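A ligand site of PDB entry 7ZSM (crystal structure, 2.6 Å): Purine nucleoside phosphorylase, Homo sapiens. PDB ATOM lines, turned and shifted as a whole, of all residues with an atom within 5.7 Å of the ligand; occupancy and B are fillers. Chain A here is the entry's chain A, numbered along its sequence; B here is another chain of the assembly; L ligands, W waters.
Gly 32 touches the ligand (CA to O3, 3.8 Å). OH of Tyr 88 touches C1 of the ligand (3.8 Å). CB of Asn 115 touches O2 of the ligand, at 3.3 Å. C of Ala 117 touches N1 of the ligand (3.6 Å). O of Pro 198 touches C9 of the ligand (3.8 Å). Phe 200 touches the ligand. Gly 218 touches the ligand (CA to N2, 3.6 Å). Met 219 touches the ligand (CG to N2, 3.9 Å). OG1 of Thr 242 touches C6 of the ligand, at 3.2 Å. Val 245 touches the ligand. His 257 touches the ligand (CD2 to C11, 3.8 Å). Phe 159 of chain B touches the ligand. Hydrophobic or aromatic side chains within 4 Å of the ligand: Ala 116, Phe 200, Val 217, Met 219, Val 245, His 257 and Phe 159 of chain B. Within 4 Å of the ligand: Gly 32, Ser 33, Arg 84, His 86, Tyr 88, Asn 115, Ala 116, Ala 117, Gly 118, Pro 198, Phe 200, Glu 201, Val 217, Gly 218, Met 219, Ser 220, Thr 242, Asn 243, Val 245, His 257 and Phe 159 of chain B.
The side-chain hydroxyl (OG1) of Thr 221 lies within hydrogen-bond range of the guanidinium group (NH1) of Arg 84. The backbone NH (N) of Ser 220 is in hydrogen-bond range of the side-chain hydroxyl (OH) of Tyr 192 (3.1 Å). N of Thr 242 lies within hydrogen-bond range of O of Ala 117, 3.0 Å away. OG of Ser 220 lies within hydrogen-bond range of OG1 of Thr 221 (2.9 Å). N of Gly 118 lies within hydrogen-bond range of O of Val 217 (2.9 Å). The side-chain hydroxyl of Thr 114 sits at hydrogen-bond distance from the backbone NH of Gly 32, 2.5 Å away. A ring nitrogen (ND1) of His 86 lies within hydrogen-bond range of the side-chain hydroxyl (OH) of Tyr 88 (3.2 Å). The backbone NH (N) of Ala 116 sits close to the side-chain hydroxyl (OG) of Ser 33, at 3.2 Å.
Water W2 lies within hydrogen-bond range of O2 of the ligand, O of Ala 116, OH of Tyr 192, N of Met 219 and OG of Ser 220.
A nitrogen (N2) of the ligand lies close to the backbone carbonyl oxygen of Val 217. N1 of the ligand is in hydrogen-bond range of OD1 of Asn 243 (3.1 Å). An oxygen (O3) of the ligand sits at hydrogen-bond distance from the backbone NH (N) of Ser 33. NE of Arg 84 lies within salt-bridge range of O4 of the ligand. OG of Ser 220 sits at hydrogen-bond distance from O2 of the ligand (2.5 Å). N of Gly 118 sits close to N1 of the ligand (3.3 Å). A nitrogen (N3) of the ligand is in hydrogen-bond range of the side-chain carboxylate (OE2) of Glu 201. NE2 of His 86 sits at hydrogen-bond distance from O4 of the ligand (3.2 Å). N of Ala 116 lies within hydrogen-bond range of O3 of the ligand (3.0 Å).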
ATOM      1  N   CYS A  31      11.076   7.239 -19.195  1.00  0.00           N
ATOM      2  CA  CYS A  31      12.251   8.028 -18.778  1.00  0.00           C
ATOM      3  C   CYS A  31      12.844   8.730 -19.989  1.00  0.00           C
ATOM      4  O   CYS A  31      13.371   8.046 -20.887  1.00  0.00           O
ATOM      5  CB  CYS A  31      13.263   7.153 -18.060  1.00  0.00           C
ATOM      6  SG  CYS A  31      12.510   6.192 -16.711  1.00  0.00           S
ATOM      7  N   GLY A  32      12.722  10.051 -20.030  1.00  0.00           N
ATOM      8  CA  GLY A  32      13.386  10.922 -21.027  1.00  0.00           C
ATOM      9  C   GLY A  32      14.731  11.400 -20.529  1.00  0.00           C
ATOM     10  O   GLY A  32      15.238  10.846 -19.524  1.00  0.00           O
ATOM     11  N   SER A  33      15.286  12.417 -21.198  1.00  0.00           N
ATOM     12  CA  SER A  33      16.659  12.949 -21.007  1.00  0.00           C
ATOM     13  C   SER A  33      17.052  12.956 -19.520  1.00  0.00           C
ATOM     14  O   SER A  33      16.399  13.665 -18.711  1.00  0.00           O
ATOM     15  CB  SER A  33      16.804  14.313 -21.611  1.00  0.00           C
ATOM     16  OG  SER A  33      15.933  15.237 -20.976  1.00  0.00           O
ATOM     17  N   ARG A  84      13.004   5.146 -25.607  1.00  0.00           N
ATOM     18  CA  ARG A  84      11.699   5.633 -26.088  1.00  0.00           C
ATOM     19  C   ARG A  84      11.734   5.608 -27.614  1.00  0.00           C
ATOM     20  O   ARG A  84      12.831   5.558 -28.178  1.00  0.00           O
ATOM     21  CB  ARG A  84      11.434   7.016 -25.501  1.00  0.00           C
ATOM     22  CG  ARG A  84      10.873   8.026 -26.491  1.00  0.00           C
ATOM     23  CD  ARG A  84       9.754   8.810 -25.840  1.00  0.00           C
ATOM     24  NE  ARG A  84      10.256   9.593 -24.731  1.00  0.00           N
ATOM     25  CZ  ARG A  84       9.494  10.316 -23.928  1.00  0.00           C
ATOM     26  NH1 ARG A  84       8.174  10.347 -24.100  1.00  0.00           N
ATOM     27  NH2 ARG A  84      10.043  10.998 -22.954  1.00  0.00           N
ATOM     28  N   HIS A  86      10.594   7.562 -31.190  1.00  0.00           N
ATOM     29  CA  HIS A  86      10.293   8.922 -31.681  1.00  0.00           C
ATOM     30  C   HIS A  86       9.896   8.901 -33.159  1.00  0.00           C
ATOM     31  O   HIS A  86      10.483   8.117 -33.935  1.00  0.00           O
ATOM     32  CB  HIS A  86      11.506   9.837 -31.479  1.00  0.00           C
ATOM     33  CG  HIS A  86      12.101   9.825 -30.110  1.00  0.00           C
ATOM     34  ND1 HIS A  86      13.156   8.993 -29.772  1.00  0.00           N
ATOM     35  CD2 HIS A  86      11.856  10.576 -29.020  1.00  0.00           C
ATOM     36  CE1 HIS A  86      13.504   9.216 -28.529  1.00  0.00           C
ATOM     37  NE2 HIS A  86      12.721  10.189 -28.044  1.00  0.00           N
ATOM     38  N   TYR A  88      10.853  10.934 -35.418  1.00  0.00           N
ATOM     39  CA  TYR A  88      12.074  11.207 -36.233  1.00  0.00           C
ATOM     40  C   TYR A  88      12.794   9.894 -36.543  1.00  0.00           C
ATOM     41  O   TYR A  88      13.364   9.819 -37.616  1.00  0.00           O
ATOM     42  CB  TYR A  88      12.997  12.254 -35.608  1.00  0.00           C
ATOM     43  CG  TYR A  88      13.622  11.923 -34.275  1.00  0.00           C
ATOM     44  CD1 TYR A  88      14.641  10.993 -34.156  1.00  0.00           C
ATOM     45  CD2 TYR A  88      13.234  12.610 -33.141  1.00  0.00           C
ATOM     46  CE1 TYR A  88      15.234  10.734 -32.923  1.00  0.00           C
ATOM     47  CE2 TYR A  88      13.812  12.360 -31.909  1.00  0.00           C
ATOM     48  CZ  TYR A  88      14.819  11.422 -31.798  1.00  0.00           C
ATOM     49  OH  TYR A  88      15.369  11.191 -30.567  1.00  0.00           O
ATOM     50  N   THR A 114       8.569  12.004 -18.792  1.00  0.00           N
ATOM     51  CA  THR A 114       9.633  13.043 -18.715  1.00  0.00           C
ATOM     52  C   THR A 114      10.161  13.267 -20.123  1.00  0.00           C
ATOM     53  O   THR A 114       9.981  12.388 -20.953  1.00  0.00           O
ATOM     54  CB  THR A 114      10.741  12.611 -17.757  1.00  0.00           C
ATOM     55  OG1 THR A 114      11.479  11.572 -18.409  1.00  0.00           O
ATOM     56  CG2 THR A 114      10.195  12.108 -16.440  1.00  0.00           C
ATOM     57  N   ASN A 115      10.857  14.373 -20.370  1.00  0.00           N
ATOM     58  CA  ASN A 115      11.385  14.682 -21.723  1.00  0.00           C
ATOM     59  C   ASN A 115      12.317  15.896 -21.678  1.00  0.00           C
ATOM     60  O   ASN A 115      12.108  16.757 -20.818  1.00  0.00           O
ATOM     61  CB  ASN A 115      10.230  14.942 -22.693  1.00  0.00           C
ATOM     62  CG  ASN A 115       9.473  16.228 -22.432  1.00  0.00           C
ATOM     63  OD1 ASN A 115      10.038  17.305 -22.485  1.00  0.00           O
ATOM     64  ND2 ASN A 115       8.172  16.122 -22.220  1.00  0.00           N
ATOM     65  N   ALA A 116      13.243  15.991 -22.633  1.00  0.00           N
ATOM     66  CA  ALA A 116      13.985  17.246 -22.887  1.00  0.00           C
ATOM     67  C   ALA A 116      13.086  18.179 -23.694  1.00  0.00           C
ATOM     68  O   ALA A 116      12.078  17.712 -24.242  1.00  0.00           O
ATOM     69  CB  ALA A 116      15.294  17.016 -23.597  1.00  0.00           C
ATOM     70  N   ALA A 117      13.473  19.446 -23.772  1.00  0.00           N
ATOM     71  CA  ALA A 117      12.751  20.490 -24.517  1.00  0.00           C
ATOM     72  C   ALA A 117      13.623  21.752 -24.576  1.00  0.00           C
ATOM     73  O   ALA A 117      14.415  21.995 -23.643  1.00  0.00           O
ATOM     74  CB  ALA A 117      11.413  20.756 -23.874  1.00  0.00           C
ATOM     75  N   GLY A 118      13.496  22.501 -25.673  1.00  0.00           N
ATOM     76  CA  GLY A 118      14.065  23.848 -25.773  1.00  0.00           C
ATOM     77  C   GLY A 118      13.128  24.850 -25.133  1.00  0.00           C
ATOM     78  O   GLY A 118      11.899  24.675 -25.285  1.00  0.00           O
ATOM     79  N   TYR A 192       3.772  22.456 -23.703  1.00  0.00           N
ATOM     80  CA  TYR A 192       4.789  21.749 -24.509  1.00  0.00           C
ATOM     81  C   TYR A 192       4.214  21.550 -25.917  1.00  0.00           C
ATOM     82  O   TYR A 192       3.139  20.936 -26.026  1.00  0.00           O
ATOM     83  CB  TYR A 192       5.114  20.425 -23.814  1.00  0.00           C
ATOM     84  CG  TYR A 192       6.000  19.465 -24.567  1.00  0.00           C
ATOM     85  CD1 TYR A 192       5.479  18.602 -25.515  1.00  0.00           C
ATOM     86  CD2 TYR A 192       7.358  19.384 -24.291  1.00  0.00           C
ATOM     87  CE1 TYR A 192       6.270  17.682 -26.177  1.00  0.00           C
ATOM     88  CE2 TYR A 192       8.170  18.475 -24.949  1.00  0.00           C
ATOM     89  CZ  TYR A 192       7.631  17.625 -25.906  1.00  0.00           C
ATOM     90  OH  TYR A 192       8.402  16.709 -26.556  1.00  0.00           O
ATOM     91  N   PRO A 198      13.845  15.472 -37.185  1.00  0.00           N
ATOM     92  CA  PRO A 198      14.812  15.623 -36.094  1.00  0.00           C
ATOM     93  C   PRO A 198      15.688  16.883 -36.097  1.00  0.00           C
ATOM     94  O   PRO A 198      16.382  17.098 -35.120  1.00  0.00           O
ATOM     95  CB  PRO A 198      15.733  14.422 -36.367  1.00  0.00           C
ATOM     96  CG  PRO A 198      15.780  14.355 -37.867  1.00  0.00           C
ATOM     97  CD  PRO A 198      14.387  14.714 -38.322  1.00  0.00           C
ATOM     98  N   SER A 199      15.664  17.673 -37.163  1.00  0.00           N
ATOM     99  CA  SER A 199      16.424  18.942 -37.266  1.00  0.00           C
ATOM    100  C   SER A 199      15.882  19.921 -36.217  1.00  0.00           C
ATOM    101  O   SER A 199      14.683  19.849 -35.880  1.00  0.00           O
ATOM    102  CB  SER A 199      16.351  19.505 -38.663  1.00  0.00           C
ATOM    103  OG  SER A 199      15.149  20.233 -38.863  1.00  0.00           O
ATOM    104  N   PHE A 200      16.751  20.790 -35.698  1.00  0.00           N
ATOM    105  CA  PHE A 200      16.386  21.861 -34.725  1.00  0.00           C
ATOM    106  C   PHE A 200      15.632  22.970 -35.476  1.00  0.00           C
ATOM    107  O   PHE A 200      15.700  23.020 -36.730  1.00  0.00           O
ATOM    108  CB  PHE A 200      17.627  22.394 -33.994  1.00  0.00           C
ATOM    109  CG  PHE A 200      18.157  21.552 -32.866  1.00  0.00           C
ATOM    110  CD1 PHE A 200      17.597  21.623 -31.597  1.00  0.00           C
ATOM    111  CD2 PHE A 200      19.262  20.732 -33.042  1.00  0.00           C
ATOM    112  CE1 PHE A 200      18.111  20.876 -30.545  1.00  0.00           C
ATOM    113  CE2 PHE A 200      19.776  19.977 -31.994  1.00  0.00           C
ATOM    114  CZ  PHE A 200      19.203  20.056 -30.750  1.00  0.00           C
ATOM    115  N   GLU A 201      14.956  23.848 -34.737  1.00  0.00           N
ATOM    116  CA  GLU A 201      14.065  24.890 -35.306  1.00  0.00           C
ATOM    117  C   GLU A 201      14.900  25.991 -35.954  1.00  0.00           C
ATOM    118  O   GLU A 201      16.006  26.271 -35.456  1.00  0.00           O
ATOM    119  CB  GLU A 201      13.160  25.499 -34.238  1.00  0.00           C
ATOM    120  CG  GLU A 201      12.006  24.612 -33.863  1.00  0.00           C
ATOM    121  CD  GLU A 201      12.484  23.382 -33.123  1.00  0.00           C
ATOM    122  OE1 GLU A 201      12.234  22.256 -33.585  1.00  0.00           O
ATOM    123  OE2 GLU A 201      13.188  23.582 -32.133  1.00  0.00           O
ATOM    124  N   VAL A 217       9.436  23.297 -26.547  1.00  0.00           N
ATOM    125  CA  VAL A 217       9.345  22.464 -27.781  1.00  0.00           C
ATOM    126  C   VAL A 217      10.233  21.223 -27.595  1.00  0.00           C
ATOM    127  O   VAL A 217      11.408  21.378 -27.276  1.00  0.00           O
ATOM    128  CB  VAL A 217       9.731  23.239 -29.055  1.00  0.00           C
ATOM    129  CG1 VAL A 217      11.157  23.758 -29.031  1.00  0.00           C
ATOM    130  CG2 VAL A 217       9.497  22.400 -30.309  1.00  0.00           C
ATOM    131  N   GLY A 218       9.652  20.034 -27.801  1.00  0.00           N
ATOM    132  CA  GLY A 218      10.360  18.742 -27.798  1.00  0.00           C
ATOM    133  C   GLY A 218       9.769  17.831 -28.857  1.00  0.00           C
ATOM    134  O   GLY A 218       8.928  18.307 -29.622  1.00  0.00           O
ATOM    135  N   MET A 219      10.166  16.561 -28.901  1.00  0.00           N
ATOM    136  CA  MET A 219       9.919  15.698 -30.072  1.00  0.00           C
ATOM    137  C   MET A 219       9.315  14.370 -29.634  1.00  0.00           C
ATOM    138  O   MET A 219       9.527  13.355 -30.334  1.00  0.00           O
ATOM    139  CB  MET A 219      11.231  15.440 -30.818  1.00  0.00           C
ATOM    140  CG  MET A 219      11.922  16.701 -31.257  1.00  0.00           C
ATOM    141  SD  MET A 219      13.368  16.357 -32.263  1.00  0.00           S
ATOM    142  CE  MET A 219      13.628  17.976 -32.982  1.00  0.00           C
ATOM    143  N   SER A 220       8.532  14.367 -28.555  1.00  0.00           N
ATOM    144  CA  SER A 220       8.034  13.123 -27.929  1.00  0.00           C
ATOM    145  C   SER A 220       6.797  13.365 -27.075  1.00  0.00           C
ATOM    146  O   SER A 220       6.180  14.424 -27.201  1.00  0.00           O
ATOM    147  CB  SER A 220       9.114  12.571 -27.083  1.00  0.00           C
ATOM    148  OG  SER A 220       9.177  13.320 -25.888  1.00  0.00           O
ATOM    149  N   THR A 221       6.456  12.385 -26.235  1.00  0.00           N
ATOM    150  CA  THR A 221       5.492  12.488 -25.115  1.00  0.00           C
ATOM    151  C   THR A 221       4.035  12.557 -25.592  1.00  0.00           C
ATOM    152  O   THR A 221       3.218  11.750 -25.098  1.00  0.00           O
ATOM    153  CB  THR A 221       5.756  13.729 -24.271  1.00  0.00           C
ATOM    154  OG1 THR A 221       7.133  13.670 -23.914  1.00  0.00           O
ATOM    155  CG2 THR A 221       4.886  13.804 -23.034  1.00  0.00           C
ATOM    156  N   THR A 242      16.619  21.840 -21.632  1.00  0.00           N
ATOM    157  CA  THR A 242      18.019  21.525 -22.039  1.00  0.00           C
ATOM    158  C   THR A 242      18.686  22.749 -22.682  1.00  0.00           C
ATOM    159  O   THR A 242      19.934  22.834 -22.621  1.00  0.00           O
ATOM    160  CB  THR A 242      18.069  20.301 -22.954  1.00  0.00           C
ATOM    161  OG1 THR A 242      17.059  20.463 -23.943  1.00  0.00           O
ATOM    162  CG2 THR A 242      17.870  19.001 -22.201  1.00  0.00           C
ATOM    163  N   ASN A 243      17.928  23.666 -23.286  1.00  0.00           N
ATOM    164  CA  ASN A 243      18.501  24.807 -24.038  1.00  0.00           C
ATOM    165  C   ASN A 243      17.458  25.914 -24.224  1.00  0.00           C
ATOM    166  O   ASN A 243      16.246  25.627 -24.079  1.00  0.00           O
ATOM    167  CB  ASN A 243      19.051  24.358 -25.392  1.00  0.00           C
ATOM    168  CG  ASN A 243      17.971  23.824 -26.320  1.00  0.00           C
ATOM    169  OD1 ASN A 243      18.198  22.900 -27.104  1.00  0.00           O
ATOM    170  ND2 ASN A 243      16.786  24.406 -26.270  1.00  0.00           N
ATOM    171  N   VAL A 245      15.801  28.218 -27.064  1.00  0.00           N
ATOM    172  CA  VAL A 245      15.673  28.151 -28.552  1.00  0.00           C
ATOM    173  C   VAL A 245      16.142  29.510 -29.096  1.00  0.00           C
ATOM    174  O   VAL A 245      15.571  30.543 -28.706  1.00  0.00           O
ATOM    175  CB  VAL A 245      14.255  27.783 -29.017  1.00  0.00           C
ATOM    176  CG1 VAL A 245      14.178  27.655 -30.531  1.00  0.00           C
ATOM    177  CG2 VAL A 245      13.770  26.497 -28.365  1.00  0.00           C
ATOM    178  N   ALA A 255      21.870  25.514 -31.800  1.00  0.00           N
ATOM    179  CA  ALA A 255      21.488  24.417 -30.873  1.00  0.00           C
ATOM    180  C   ALA A 255      22.328  23.185 -31.244  1.00  0.00           C
ATOM    181  O   ALA A 255      22.909  23.188 -32.343  1.00  0.00           O
ATOM    182  CB  ALA A 255      20.013  24.152 -30.946  1.00  0.00           C
ATOM    183  N   HIS A 257      22.903  18.604 -30.058  1.00  0.00           N
ATOM    184  CA  HIS A 257      22.558  17.412 -29.234  1.00  0.00           C
ATOM    185  C   HIS A 257      23.461  17.344 -27.996  1.00  0.00           C
ATOM    186  O   HIS A 257      22.936  17.012 -26.904  1.00  0.00           O
ATOM    187  CB  HIS A 257      22.598  16.136 -30.078  1.00  0.00           C
ATOM    188  CG  HIS A 257      22.047  14.954 -29.352  1.00  0.00           C
ATOM    189  ND1 HIS A 257      22.807  13.836 -29.074  1.00  0.00           N
ATOM    190  CD2 HIS A 257      20.818  14.726 -28.829  1.00  0.00           C
ATOM    191  CE1 HIS A 257      22.072  12.966 -28.410  1.00  0.00           C
ATOM    192  NE2 HIS A 257      20.851  13.489 -28.253  1.00  0.00           N
ATOM    193  N   VAL A 260      22.380  18.967 -24.989  1.00  0.00           N
ATOM    194  CA  VAL A 260      21.138  18.295 -24.500  1.00  0.00           C
ATOM    195  C   VAL A 260      21.523  17.113 -23.607  1.00  0.00           C
ATOM    196  O   VAL A 260      20.882  16.928 -22.554  1.00  0.00           O
ATOM    197  CB  VAL A 260      20.242  17.855 -25.663  1.00  0.00           C
ATOM    198  CG1 VAL A 260      19.002  17.113 -25.188  1.00  0.00           C
ATOM    199  CG2 VAL A 260      19.840  19.023 -26.552  1.00  0.00           C
ATOM    200  N   PHE B 159      20.882  15.203 -35.474  1.00  0.00           N
ATOM    201  CA  PHE B 159      20.099  16.397 -35.076  1.00  0.00           C
ATOM    202  C   PHE B 159      20.816  17.675 -35.523  1.00  0.00           C
ATOM    203  O   PHE B 159      21.278  18.465 -34.701  1.00  0.00           O
ATOM    204  CB  PHE B 159      19.860  16.398 -33.566  1.00  0.00           C
ATOM    205  CG  PHE B 159      19.279  15.132 -32.985  1.00  0.00           C
ATOM    206  CD1 PHE B 159      17.909  14.891 -33.012  1.00  0.00           C
ATOM    207  CD2 PHE B 159      20.105  14.203 -32.364  1.00  0.00           C
ATOM    208  CE1 PHE B 159      17.392  13.727 -32.453  1.00  0.00           C
ATOM    209  CE2 PHE B 159      19.564  13.056 -31.798  1.00  0.00           C
ATOM    210  CZ  PHE B 159      18.216  12.816 -31.849  1.00  0.00           C
HETATM  211  N1  LIG L   1      15.863  20.910 -27.232  1.00  0.00           N
HETATM  212  N2  LIG L   1      13.348  19.822 -29.462  1.00  0.00           N
HETATM  213  C1  LIG L   1      16.087  14.276 -28.431  1.00  0.00           C
HETATM  214  C2  LIG L   1      15.136  15.082 -27.794  1.00  0.00           C
HETATM  215  C3  LIG L   1      14.152  14.496 -26.876  1.00  0.00           C
HETATM  216  C4  LIG L   1      13.994  13.222 -26.544  1.00  0.00           C
HETATM  217  C5  LIG L   1      15.126  16.453 -28.034  1.00  0.00           C
HETATM  218  C6  LIG L   1      15.604  19.682 -26.719  1.00  0.00           C
HETATM  219  C7  LIG L   1      13.220  20.822 -30.275  1.00  0.00           C
HETATM  220  C8  LIG L   1      16.054  17.001 -28.899  1.00  0.00           C
HETATM  221  C9  LIG L   1      17.324  17.502 -31.454  1.00  0.00           C
HETATM  222  O1  LIG L   1      17.894  16.769 -30.369  1.00  0.00           O
HETATM  223  C10 LIG L   1      17.004  16.195 -29.511  1.00  0.00           C
HETATM  224  C11 LIG L   1      17.014  14.833 -29.292  1.00  0.00           C
HETATM  225  P1  LIG L   1      12.946  12.864 -25.221  1.00  0.00           P
HETATM  226  O2  LIG L   1      11.641  13.585 -25.377  1.00  0.00           O
HETATM  227  O3  LIG L   1      13.603  13.288 -23.944  1.00  0.00           O
HETATM  228  O4  LIG L   1      12.652  11.406 -25.132  1.00  0.00           O
HETATM  229  S1  LIG L   1      13.926  17.508 -27.241  1.00  0.00           S
HETATM  230  C12 LIG L   1      14.620  19.094 -27.468  1.00  0.00           C
HETATM  231  C13 LIG L   1      15.057  21.111 -28.320  1.00  0.00           C
HETATM  232  C14 LIG L   1      14.910  22.201 -29.222  1.00  0.00           C
HETATM  233  O5  LIG L   1      15.528  23.277 -29.208  1.00  0.00           O
HETATM  234  N3  LIG L   1      13.935  21.953 -30.187  1.00  0.00           N
HETATM  235  C15 LIG L   1      14.273  19.967 -28.470  1.00  0.00           C
HETATM  236  O   HOH W   1      18.226  12.146 -27.256  1.00  0.00           O
HETATM  237  O   HOH W   2      11.157  15.872 -26.019  1.00  0.00           O
